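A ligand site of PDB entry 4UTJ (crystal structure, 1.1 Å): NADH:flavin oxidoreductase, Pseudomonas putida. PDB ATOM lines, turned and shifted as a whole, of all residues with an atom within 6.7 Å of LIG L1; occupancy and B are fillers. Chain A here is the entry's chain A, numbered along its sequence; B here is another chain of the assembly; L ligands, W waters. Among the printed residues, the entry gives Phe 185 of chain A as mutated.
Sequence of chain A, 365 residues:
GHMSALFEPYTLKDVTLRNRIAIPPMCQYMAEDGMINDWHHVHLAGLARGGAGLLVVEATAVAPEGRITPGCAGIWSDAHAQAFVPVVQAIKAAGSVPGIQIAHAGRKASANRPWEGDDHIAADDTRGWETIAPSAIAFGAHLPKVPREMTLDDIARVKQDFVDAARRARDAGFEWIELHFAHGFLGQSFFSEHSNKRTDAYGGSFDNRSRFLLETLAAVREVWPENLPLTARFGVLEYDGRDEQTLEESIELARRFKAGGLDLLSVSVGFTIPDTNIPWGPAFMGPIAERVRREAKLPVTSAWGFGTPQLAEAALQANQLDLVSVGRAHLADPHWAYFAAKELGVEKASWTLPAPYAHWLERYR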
ATOM      1  N   PRO A  25      17.734  18.993 -15.415  1.00  0.00           N
ATOM      2  CA  PRO A  25      16.856  17.973 -15.986  1.00  0.00           C
ATOM      3  C   PRO A  25      15.542  17.906 -15.219  1.00  0.00           C
ATOM      4  O   PRO A  25      15.519  17.842 -13.997  1.00  0.00           O
ATOM      5  CB  PRO A  25      17.680  16.680 -15.847  1.00  0.00           C
ATOM      6  CG  PRO A  25      18.660  16.972 -14.727  1.00  0.00           C
ATOM      7  CD  PRO A  25      19.001  18.429 -14.922  1.00  0.00           C
ATOM      8  N   MET A  26      14.431  17.886 -15.967  1.00  0.00           N
ATOM      9  CA  MET A  26      13.097  17.753 -15.390  1.00  0.00           C
ATOM     10  C   MET A  26      12.260  16.821 -16.256  1.00  0.00           C
ATOM     11  O   MET A  26      11.709  17.204 -17.293  1.00  0.00           O
ATOM     12  CB  MET A  26      12.393  19.113 -15.243  1.00  0.00           C
ATOM     13  CG  MET A  26      12.989  19.965 -14.131  1.00  0.00           C
ATOM     14  SD  MET A  26      12.106  21.512 -13.864  1.00  0.00           S
ATOM     15  CE  MET A  26      12.684  22.381 -15.309  1.00  0.00           C
ATOM     16  N   CYS A  27      12.115  15.613 -15.776  1.00  0.00           N
ATOM     17  CA  CYS A  27      11.240  14.629 -16.397  1.00  0.00           C
ATOM     18  C   CYS A  27       9.857  15.188 -16.687  1.00  0.00           C
ATOM     19  O   CYS A  27       9.227  15.859 -15.834  1.00  0.00           O
ATOM     20  CB  CYS A  27      11.111  13.401 -15.517  1.00  0.00           C
ATOM     21  SG  CYS A  27      12.482  12.261 -15.586  1.00  0.00           S
ATOM     22  N   TYR A  29       7.485  12.899 -18.411  1.00  0.00           N
ATOM     23  CA  TYR A  29       6.608  11.746 -18.401  1.00  0.00           C
ATOM     24  C   TYR A  29       5.666  11.686 -19.599  1.00  0.00           C
ATOM     25  O   TYR A  29       4.565  11.147 -19.499  1.00  0.00           O
ATOM     26  CB  TYR A  29       5.838  11.619 -17.067  1.00  0.00           C
ATOM     27  CG  TYR A  29       6.712  11.800 -15.851  1.00  0.00           C
ATOM     28  CD1 TYR A  29       7.359  10.710 -15.282  1.00  0.00           C
ATOM     29  CD2 TYR A  29       6.930  13.046 -15.297  1.00  0.00           C
ATOM     30  CE1 TYR A  29       8.195  10.864 -14.174  1.00  0.00           C
ATOM     31  CE2 TYR A  29       7.772  13.201 -14.201  1.00  0.00           C
ATOM     32  CZ  TYR A  29       8.376  12.113 -13.638  1.00  0.00           C
ATOM     33  OH  TYR A  29       9.181  12.301 -12.558  1.00  0.00           O
ATOM     34  N   ALA A  59      16.119  13.272 -17.375  1.00  0.00           N
ATOM     35  CA  ALA A  59      16.645  11.911 -17.254  1.00  0.00           C
ATOM     36  C   ALA A  59      16.172  11.074 -18.438  1.00  0.00           C
ATOM     37  O   ALA A  59      14.975  10.800 -18.589  1.00  0.00           O
ATOM     38  CB  ALA A  59      16.184  11.290 -15.966  1.00  0.00           C
ATOM     39  N   ILE A  68      12.278   5.519 -15.282  1.00  0.00           N
ATOM     40  CA  ILE A  68      11.517   5.552 -14.039  1.00  0.00           C
ATOM     41  C   ILE A  68      10.108   5.024 -14.285  1.00  0.00           C
ATOM     42  O   ILE A  68       9.595   4.229 -13.496  1.00  0.00           O
ATOM     43  CB  ILE A  68      11.480   6.984 -13.434  1.00  0.00           C
ATOM     44  CG1 ILE A  68      12.883   7.563 -13.312  1.00  0.00           C
ATOM     45  CG2 ILE A  68      10.775   6.924 -12.094  1.00  0.00           C
ATOM     46  CD1 ILE A  68      12.874   9.078 -13.112  1.00  0.00           C
ATOM     47  N   GLN A 101      20.790  14.635 -19.582  1.00  0.00           N
ATOM     48  CA  GLN A 101      21.088  13.748 -18.463  1.00  0.00           C
ATOM     49  C   GLN A 101      20.759  12.320 -18.882  1.00  0.00           C
ATOM     50  O   GLN A 101      19.617  12.032 -19.228  1.00  0.00           O
ATOM     51  CB  GLN A 101      20.273  14.153 -17.235  1.00  0.00           C
ATOM     52  CG  GLN A 101      20.677  13.367 -16.030  1.00  0.00           C
ATOM     53  CD  GLN A 101      19.735  13.577 -14.860  1.00  0.00           C
ATOM     54  OE1 GLN A 101      18.551  13.283 -14.982  1.00  0.00           O
ATOM     55  NE2 GLN A 101      20.250  14.069 -13.742  1.00  0.00           N
ATOM     56  N   PRO A 114       4.010  10.642 -11.671  1.00  0.00           N
ATOM     57  CA  PRO A 114       3.769  11.235 -10.352  1.00  0.00           C
ATOM     58  C   PRO A 114       2.306  11.600 -10.075  1.00  0.00           C
ATOM     59  O   PRO A 114       1.884  11.547  -8.936  1.00  0.00           O
ATOM     60  CB  PRO A 114       4.684  12.449 -10.353  1.00  0.00           C
ATOM     61  CG  PRO A 114       5.822  12.025 -11.252  1.00  0.00           C
ATOM     62  CD  PRO A 114       5.144  11.285 -12.353  1.00  0.00           C
ATOM     63  N   HIS A 180      23.549  10.565 -14.514  1.00  0.00           N
ATOM     64  CA  HIS A 180      22.652  10.626 -13.367  1.00  0.00           C
ATOM     65  C   HIS A 180      23.034   9.602 -12.314  1.00  0.00           C
ATOM     66  O   HIS A 180      22.536   8.475 -12.298  1.00  0.00           O
ATOM     67  CB  HIS A 180      21.212  10.419 -13.788  1.00  0.00           C
ATOM     68  CG  HIS A 180      20.250  10.848 -12.740  1.00  0.00           C
ATOM     69  ND1 HIS A 180      20.645  11.208 -11.464  1.00  0.00           N
ATOM     70  CD2 HIS A 180      18.910  11.047 -12.814  1.00  0.00           C
ATOM     71  CE1 HIS A 180      19.576  11.637 -10.824  1.00  0.00           C
ATOM     72  NE2 HIS A 180      18.510  11.567 -11.619  1.00  0.00           N
ATOM     73  N   ALA A 182      22.605  10.270  -9.058  1.00  0.00           N
ATOM     74  CA  ALA A 182      21.966  10.791  -7.861  1.00  0.00           C
ATOM     75  C   ALA A 182      20.588  10.163  -7.636  1.00  0.00           C
ATOM     76  O   ALA A 182      20.119   9.303  -8.394  1.00  0.00           O
ATOM     77  CB  ALA A 182      21.898  12.324  -7.940  1.00  0.00           C
ATOM     78  N   HIS A 183      19.941  10.586  -6.554  1.00  0.00           N
ATOM     79  CA  HIS A 183      18.497  10.446  -6.354  1.00  0.00           C
ATOM     80  C   HIS A 183      18.040   9.011  -6.198  1.00  0.00           C
ATOM     81  O   HIS A 183      16.880   8.680  -6.415  1.00  0.00           O
ATOM     82  CB  HIS A 183      17.720  11.216  -7.434  1.00  0.00           C
ATOM     83  CG  HIS A 183      18.042  12.677  -7.449  1.00  0.00           C
ATOM     84  ND1 HIS A 183      17.640  13.508  -8.475  1.00  0.00           N
ATOM     85  CD2 HIS A 183      18.729  13.469  -6.582  1.00  0.00           C
ATOM     86  CE1 HIS A 183      18.060  14.734  -8.235  1.00  0.00           C
ATOM     87  NE2 HIS A 183      18.727  14.745  -7.088  1.00  0.00           N
ATOM     88  N   PHE A 185      18.809   6.302  -7.702  1.00  0.00           N
ATOM     89  CA  PHE A 185      18.766   5.512  -8.917  1.00  0.00           C
ATOM     90  C   PHE A 185      19.998   4.614  -8.978  1.00  0.00           C
ATOM     91  O   PHE A 185      20.687   4.420  -7.965  1.00  0.00           O
ATOM     92  CB  PHE A 185      18.591   6.450 -10.099  1.00  0.00           C
ATOM     93  CG  PHE A 185      17.288   7.232 -10.085  1.00  0.00           C
ATOM     94  CD1 PHE A 185      16.062   6.626  -9.910  1.00  0.00           C
ATOM     95  CD2 PHE A 185      17.317   8.590 -10.275  1.00  0.00           C
ATOM     96  CE1 PHE A 185      14.895   7.337  -9.930  1.00  0.00           C
ATOM     97  CE2 PHE A 185      16.143   9.329 -10.304  1.00  0.00           C
ATOM     98  CZ  PHE A 185      14.928   8.701 -10.150  1.00  0.00           C
ATOM     99  N   ARG A 233      25.546  14.193 -11.877  1.00  0.00           N
ATOM    100  CA  ARG A 233      24.773  14.559 -10.704  1.00  0.00           C
ATOM    101  C   ARG A 233      24.987  13.462  -9.676  1.00  0.00           C
ATOM    102  O   ARG A 233      24.960  12.275 -10.005  1.00  0.00           O
ATOM    103  CB  ARG A 233      23.279  14.720 -11.038  1.00  0.00           C
ATOM    104  CG  ARG A 233      22.518  15.531  -9.952  1.00  0.00           C
ATOM    105  CD  ARG A 233      21.147  15.984 -10.411  1.00  0.00           C
ATOM    106  NE  ARG A 233      20.786  17.226  -9.737  1.00  0.00           N
ATOM    107  CZ  ARG A 233      19.653  17.901  -9.926  1.00  0.00           C
ATOM    108  NH1 ARG A 233      18.695  17.417 -10.683  1.00  0.00           N
ATOM    109  NH2 ARG A 233      19.540  19.102  -9.372  1.00  0.00           N
ATOM    110  N   SER A 268      23.717  17.091  -5.181  1.00  0.00           N
ATOM    111  CA  SER A 268      22.373  16.871  -4.727  1.00  0.00           C
ATOM    112  C   SER A 268      22.352  16.027  -3.459  1.00  0.00           C
ATOM    113  O   SER A 268      23.364  15.847  -2.785  1.00  0.00           O
ATOM    114  CB  SER A 268      21.549  16.257  -5.873  1.00  0.00           C
ATOM    115  OG  SER A 268      20.182  16.367  -5.549  1.00  0.00           O
ATOM    116  N   PHE A 271      18.588  10.588  -1.687  1.00  0.00           N
ATOM    117  CA  PHE A 271      17.277   9.959  -1.777  1.00  0.00           C
ATOM    118  C   PHE A 271      17.364   8.438  -1.916  1.00  0.00           C
ATOM    119  O   PHE A 271      16.543   7.821  -2.587  1.00  0.00           O
ATOM    120  CB  PHE A 271      16.444  10.532  -2.942  1.00  0.00           C
ATOM    121  CG  PHE A 271      16.203  12.012  -2.850  1.00  0.00           C
ATOM    122  CD1 PHE A 271      15.277  12.529  -1.951  1.00  0.00           C
ATOM    123  CD2 PHE A 271      16.899  12.893  -3.660  1.00  0.00           C
ATOM    124  CE1 PHE A 271      15.044  13.898  -1.889  1.00  0.00           C
ATOM    125  CE2 PHE A 271      16.678  14.247  -3.587  1.00  0.00           C
ATOM    126  CZ  PHE A 271      15.752  14.759  -2.695  1.00  0.00           C
ATOM    127  N   TRP A 280      14.550  20.729   3.986  1.00  0.00           N
ATOM    128  CA  TRP A 280      14.147  21.528   2.846  1.00  0.00           C
ATOM    129  C   TRP A 280      14.040  23.005   3.200  1.00  0.00           C
ATOM    130  O   TRP A 280      13.479  23.351   4.222  1.00  0.00           O
ATOM    131  CB  TRP A 280      12.772  21.074   2.362  1.00  0.00           C
ATOM    132  CG  TRP A 280      12.686  19.625   2.043  1.00  0.00           C
ATOM    133  CD1 TRP A 280      12.072  18.648   2.782  1.00  0.00           C
ATOM    134  CD2 TRP A 280      13.235  18.973   0.908  1.00  0.00           C
ATOM    135  NE1 TRP A 280      12.197  17.437   2.161  1.00  0.00           N
ATOM    136  CE2 TRP A 280      12.927  17.605   1.017  1.00  0.00           C
ATOM    137  CE3 TRP A 280      13.980  19.418  -0.187  1.00  0.00           C
ATOM    138  CZ2 TRP A 280      13.308  16.682   0.051  1.00  0.00           C
ATOM    139  CZ3 TRP A 280      14.370  18.491  -1.125  1.00  0.00           C
ATOM    140  CH2 TRP A 280      14.027  17.157  -1.007  1.00  0.00           C
ATOM    141  N   TRP A 304      17.289  23.760  -5.755  1.00  0.00           N
ATOM    142  CA  TRP A 304      16.201  23.717  -4.774  1.00  0.00           C
ATOM    143  C   TRP A 304      16.021  25.099  -4.196  1.00  0.00           C
ATOM    144  O   TRP A 304      16.752  25.534  -3.302  1.00  0.00           O
ATOM    145  CB  TRP A 304      16.320  22.683  -3.676  1.00  0.00           C
ATOM    146  CG  TRP A 304      15.029  22.687  -2.860  1.00  0.00           C
ATOM    147  CD1 TRP A 304      14.646  23.598  -1.872  1.00  0.00           C
ATOM    148  CD2 TRP A 304      13.946  21.771  -2.991  1.00  0.00           C
ATOM    149  NE1 TRP A 304      13.413  23.272  -1.406  1.00  0.00           N
ATOM    150  CE2 TRP A 304      12.953  22.173  -2.064  1.00  0.00           C
ATOM    151  CE3 TRP A 304      13.719  20.656  -3.790  1.00  0.00           C
ATOM    152  CZ2 TRP A 304      11.750  21.483  -1.925  1.00  0.00           C
ATOM    153  CZ3 TRP A 304      12.521  19.978  -3.647  1.00  0.00           C
ATOM    154  CH2 TRP A 304      11.554  20.393  -2.714  1.00  0.00           C
ATOM    155  N   TRP B 360       3.546  19.608 -10.247  1.00  0.00           N
ATOM    156  CA  TRP B 360       4.692  20.045  -9.451  1.00  0.00           C
ATOM    157  C   TRP B 360       4.523  21.436  -8.891  1.00  0.00           C
ATOM    158  O   TRP B 360       5.256  21.830  -7.991  1.00  0.00           O
ATOM    159  CB  TRP B 360       5.947  20.021 -10.318  1.00  0.00           C
ATOM    160  CG  TRP B 360       6.186  18.693 -10.917  1.00  0.00           C
ATOM    161  CD1 TRP B 360       5.874  18.286 -12.189  1.00  0.00           C
ATOM    162  CD2 TRP B 360       6.745  17.573 -10.261  1.00  0.00           C
ATOM    163  NE1 TRP B 360       6.225  16.978 -12.345  1.00  0.00           N
ATOM    164  CE2 TRP B 360       6.794  16.517 -11.188  1.00  0.00           C
ATOM    165  CE3 TRP B 360       7.251  17.366  -8.984  1.00  0.00           C
ATOM    166  CZ2 TRP B 360       7.307  15.276 -10.856  1.00  0.00           C
ATOM    167  CZ3 TRP B 360       7.765  16.149  -8.657  1.00  0.00           C
ATOM    168  CH2 TRP B 360       7.803  15.108  -9.596  1.00  0.00           C
HETATM  169  C1  LIG L   1      12.094  13.135 -11.014  1.00  0.00           C
HETATM  170  C2  LIG L   1      12.774  12.351 -11.805  1.00  0.00           C
HETATM  171  C3  LIG L   1      14.130  12.139 -11.646  1.00  0.00           C
HETATM  172  C4  LIG L   1      14.857  12.736 -10.597  1.00  0.00           C
HETATM  173  C5  LIG L   1      14.160  13.594  -9.712  1.00  0.00           C
HETATM  174  C6  LIG L   1      12.705  13.806  -9.943  1.00  0.00           C
HETATM  175  C7  LIG L   1      12.051  14.662  -9.053  1.00  0.00           C
HETATM  176  C8  LIG L   1      12.731  15.252  -8.091  1.00  0.00           C
HETATM  177  C9  LIG L   1      14.086  15.059  -7.883  1.00  0.00           C
HETATM  178  O1  LIG L   1      14.739  14.215  -8.733  1.00  0.00           O
HETATM  179  O2  LIG L   1      14.756  15.563  -7.020  1.00  0.00           O
HETATM  180  O3  LIG L   1      16.119  12.544 -10.474  1.00  0.00           O
HETATM  181  N1  LG2 L   2      16.304  15.750 -11.261  1.00  0.00           N
HETATM  182  C1  LG2 L   2      17.114  14.984 -12.003  1.00  0.00           C
HETATM  183  O1  LG2 L   2      18.329  14.826 -11.710  1.00  0.00           O
HETATM  184  N2  LG2 L   2      16.618  14.390 -13.168  1.00  0.00           N
HETATM  185  C2  LG2 L   2      15.386  14.571 -13.641  1.00  0.00           C
HETATM  186  O2  LG2 L   2      15.035  14.158 -14.750  1.00  0.00           O
HETATM  187  C3  LG2 L   2      14.482  15.283 -12.744  1.00  0.00           C
HETATM  188  N3  LG2 L   2      13.161  15.387 -13.070  1.00  0.00           N
HETATM  189  C4  LG2 L   2      12.403  16.300 -12.367  1.00  0.00           C
HETATM  190  C5  LG2 L   2      11.101  16.602 -12.847  1.00  0.00           C
HETATM  191  C6  LG2 L   2      10.362  17.670 -12.318  1.00  0.00           C
HETATM  192  C7  LG2 L   2       9.135  18.068 -12.997  1.00  0.00           C
HETATM  193  C8  LG2 L   2      10.884  18.364 -11.210  1.00  0.00           C
HETATM  194  C9  LG2 L   2      10.128  19.471 -10.598  1.00  0.00           C
HETATM  195  C10 LG2 L   2      12.124  17.966 -10.666  1.00  0.00           C
HETATM  196  C11 LG2 L   2      12.947  17.033 -11.323  1.00  0.00           C
HETATM  197  N4  LG2 L   2      14.261  16.792 -10.911  1.00  0.00           N
HETATM  198  C12 LG2 L   2      15.027  15.905 -11.631  1.00  0.00           C
HETATM  199  C13 LG2 L   2      14.870  17.687  -9.892  1.00  0.00           C
HETATM  200  C14 LG2 L   2      15.180  19.066 -10.480  1.00  0.00           C
HETATM  201  O3  LG2 L   2      16.249  18.976 -11.428  1.00  0.00           O
HETATM  202  C15 LG2 L   2      15.616  20.072  -9.408  1.00  0.00           C
HETATM  203  O4  LG2 L   2      16.810  19.618  -8.767  1.00  0.00           O
HETATM  204  C16 LG2 L   2      14.552  20.307  -8.342  1.00  0.00           C
HETATM  205  O5  LG2 L   2      13.268  20.528  -8.923  1.00  0.00           O
HETATM  206  C17 LG2 L   2      14.896  21.462  -7.388  1.00  0.00           C
HETATM  207  O6  LG2 L   2      15.040  22.720  -8.053  1.00  0.00           O
HETATM  208  P1  LG2 L   2      13.820  23.780  -8.035  1.00  0.00           P
HETATM  209  O7  LG2 L   2      12.649  23.126  -8.737  1.00  0.00           O
HETATM  210  O8  LG2 L   2      13.498  24.085  -6.600  1.00  0.00           O
HETATM  211  O9  LG2 L   2      14.395  24.932  -8.792  1.00  0.00           O
HETATM  212  O   HOH W   1      13.696  17.493  -5.399  1.00  0.00           O
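NE2 of His 180 is in hydrogen-bond range of O1 of LG2 L2 (3.3 Å). An oxygen (O6) of LG2 L2 lies within hydrogen-bond range of the backbone NH of Trp 304 (3.4 Å). O1 of LG2 L2 sits at hydrogen-bond distance from NH1 of Arg 233, 2.8 Å away. A nitrogen (N3) of LG2 L2 is in hydrogen-bond range of the backbone NH of Cys 27 (2.9 Å). NE2 of His 180 lies within hydrogen-bond range of O3 of LIG L1 (2.8 Å). An oxygen (O3) of LIG L1 is in hydrogen-bond range of a ring nitrogen (ND1) of His 183 (2.7 Å). O3 of LG2 L2 sits at hydrogen-bond distance from O of Pro 25 (2.9 Å). The side-chain sulfur (SG) of Cys 27 is in hydrogen-bond range of an oxygen (O2) of LG2 L2 (3.3 Å). The backbone NH (N) of Ala 59 lies within hydrogen-bond range of an oxygen (O2) of LG2 L2 (3.0 Å). OE1 of Gln 101 sits at hydrogen-bond distance from N2 of LG2 L2.
O3 of LIG L1 sits close to N2 of LG2 L2 (3.3 Å).
ND1 of His 180 is in hydrogen-bond range of N of Ala 182. The side-chain hydroxyl of Ser 268 lies within hydrogen-bond range of a ring nitrogen (NE2) of His 183 (2.7 Å).
SG of Cys 27 touches C2 of LIG L1, 3.8 Å away. Tyr 29 touches LIG L1 (OH to C1, 3.4 Å). CD1 of Ile 68 touches C2 of LIG L1 (3.5 Å). Phe 185 touches LIG L1 (CE2 to O3, 3.2 Å). Hydrophobic or aromatic side chains that line LIG L1: Ile 68, His 180, His 183 and Phe 185. Within 4 Å of LIG L1: Cys 27, Tyr 29, Ile 68, His 180, His 183 and Phe 185.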
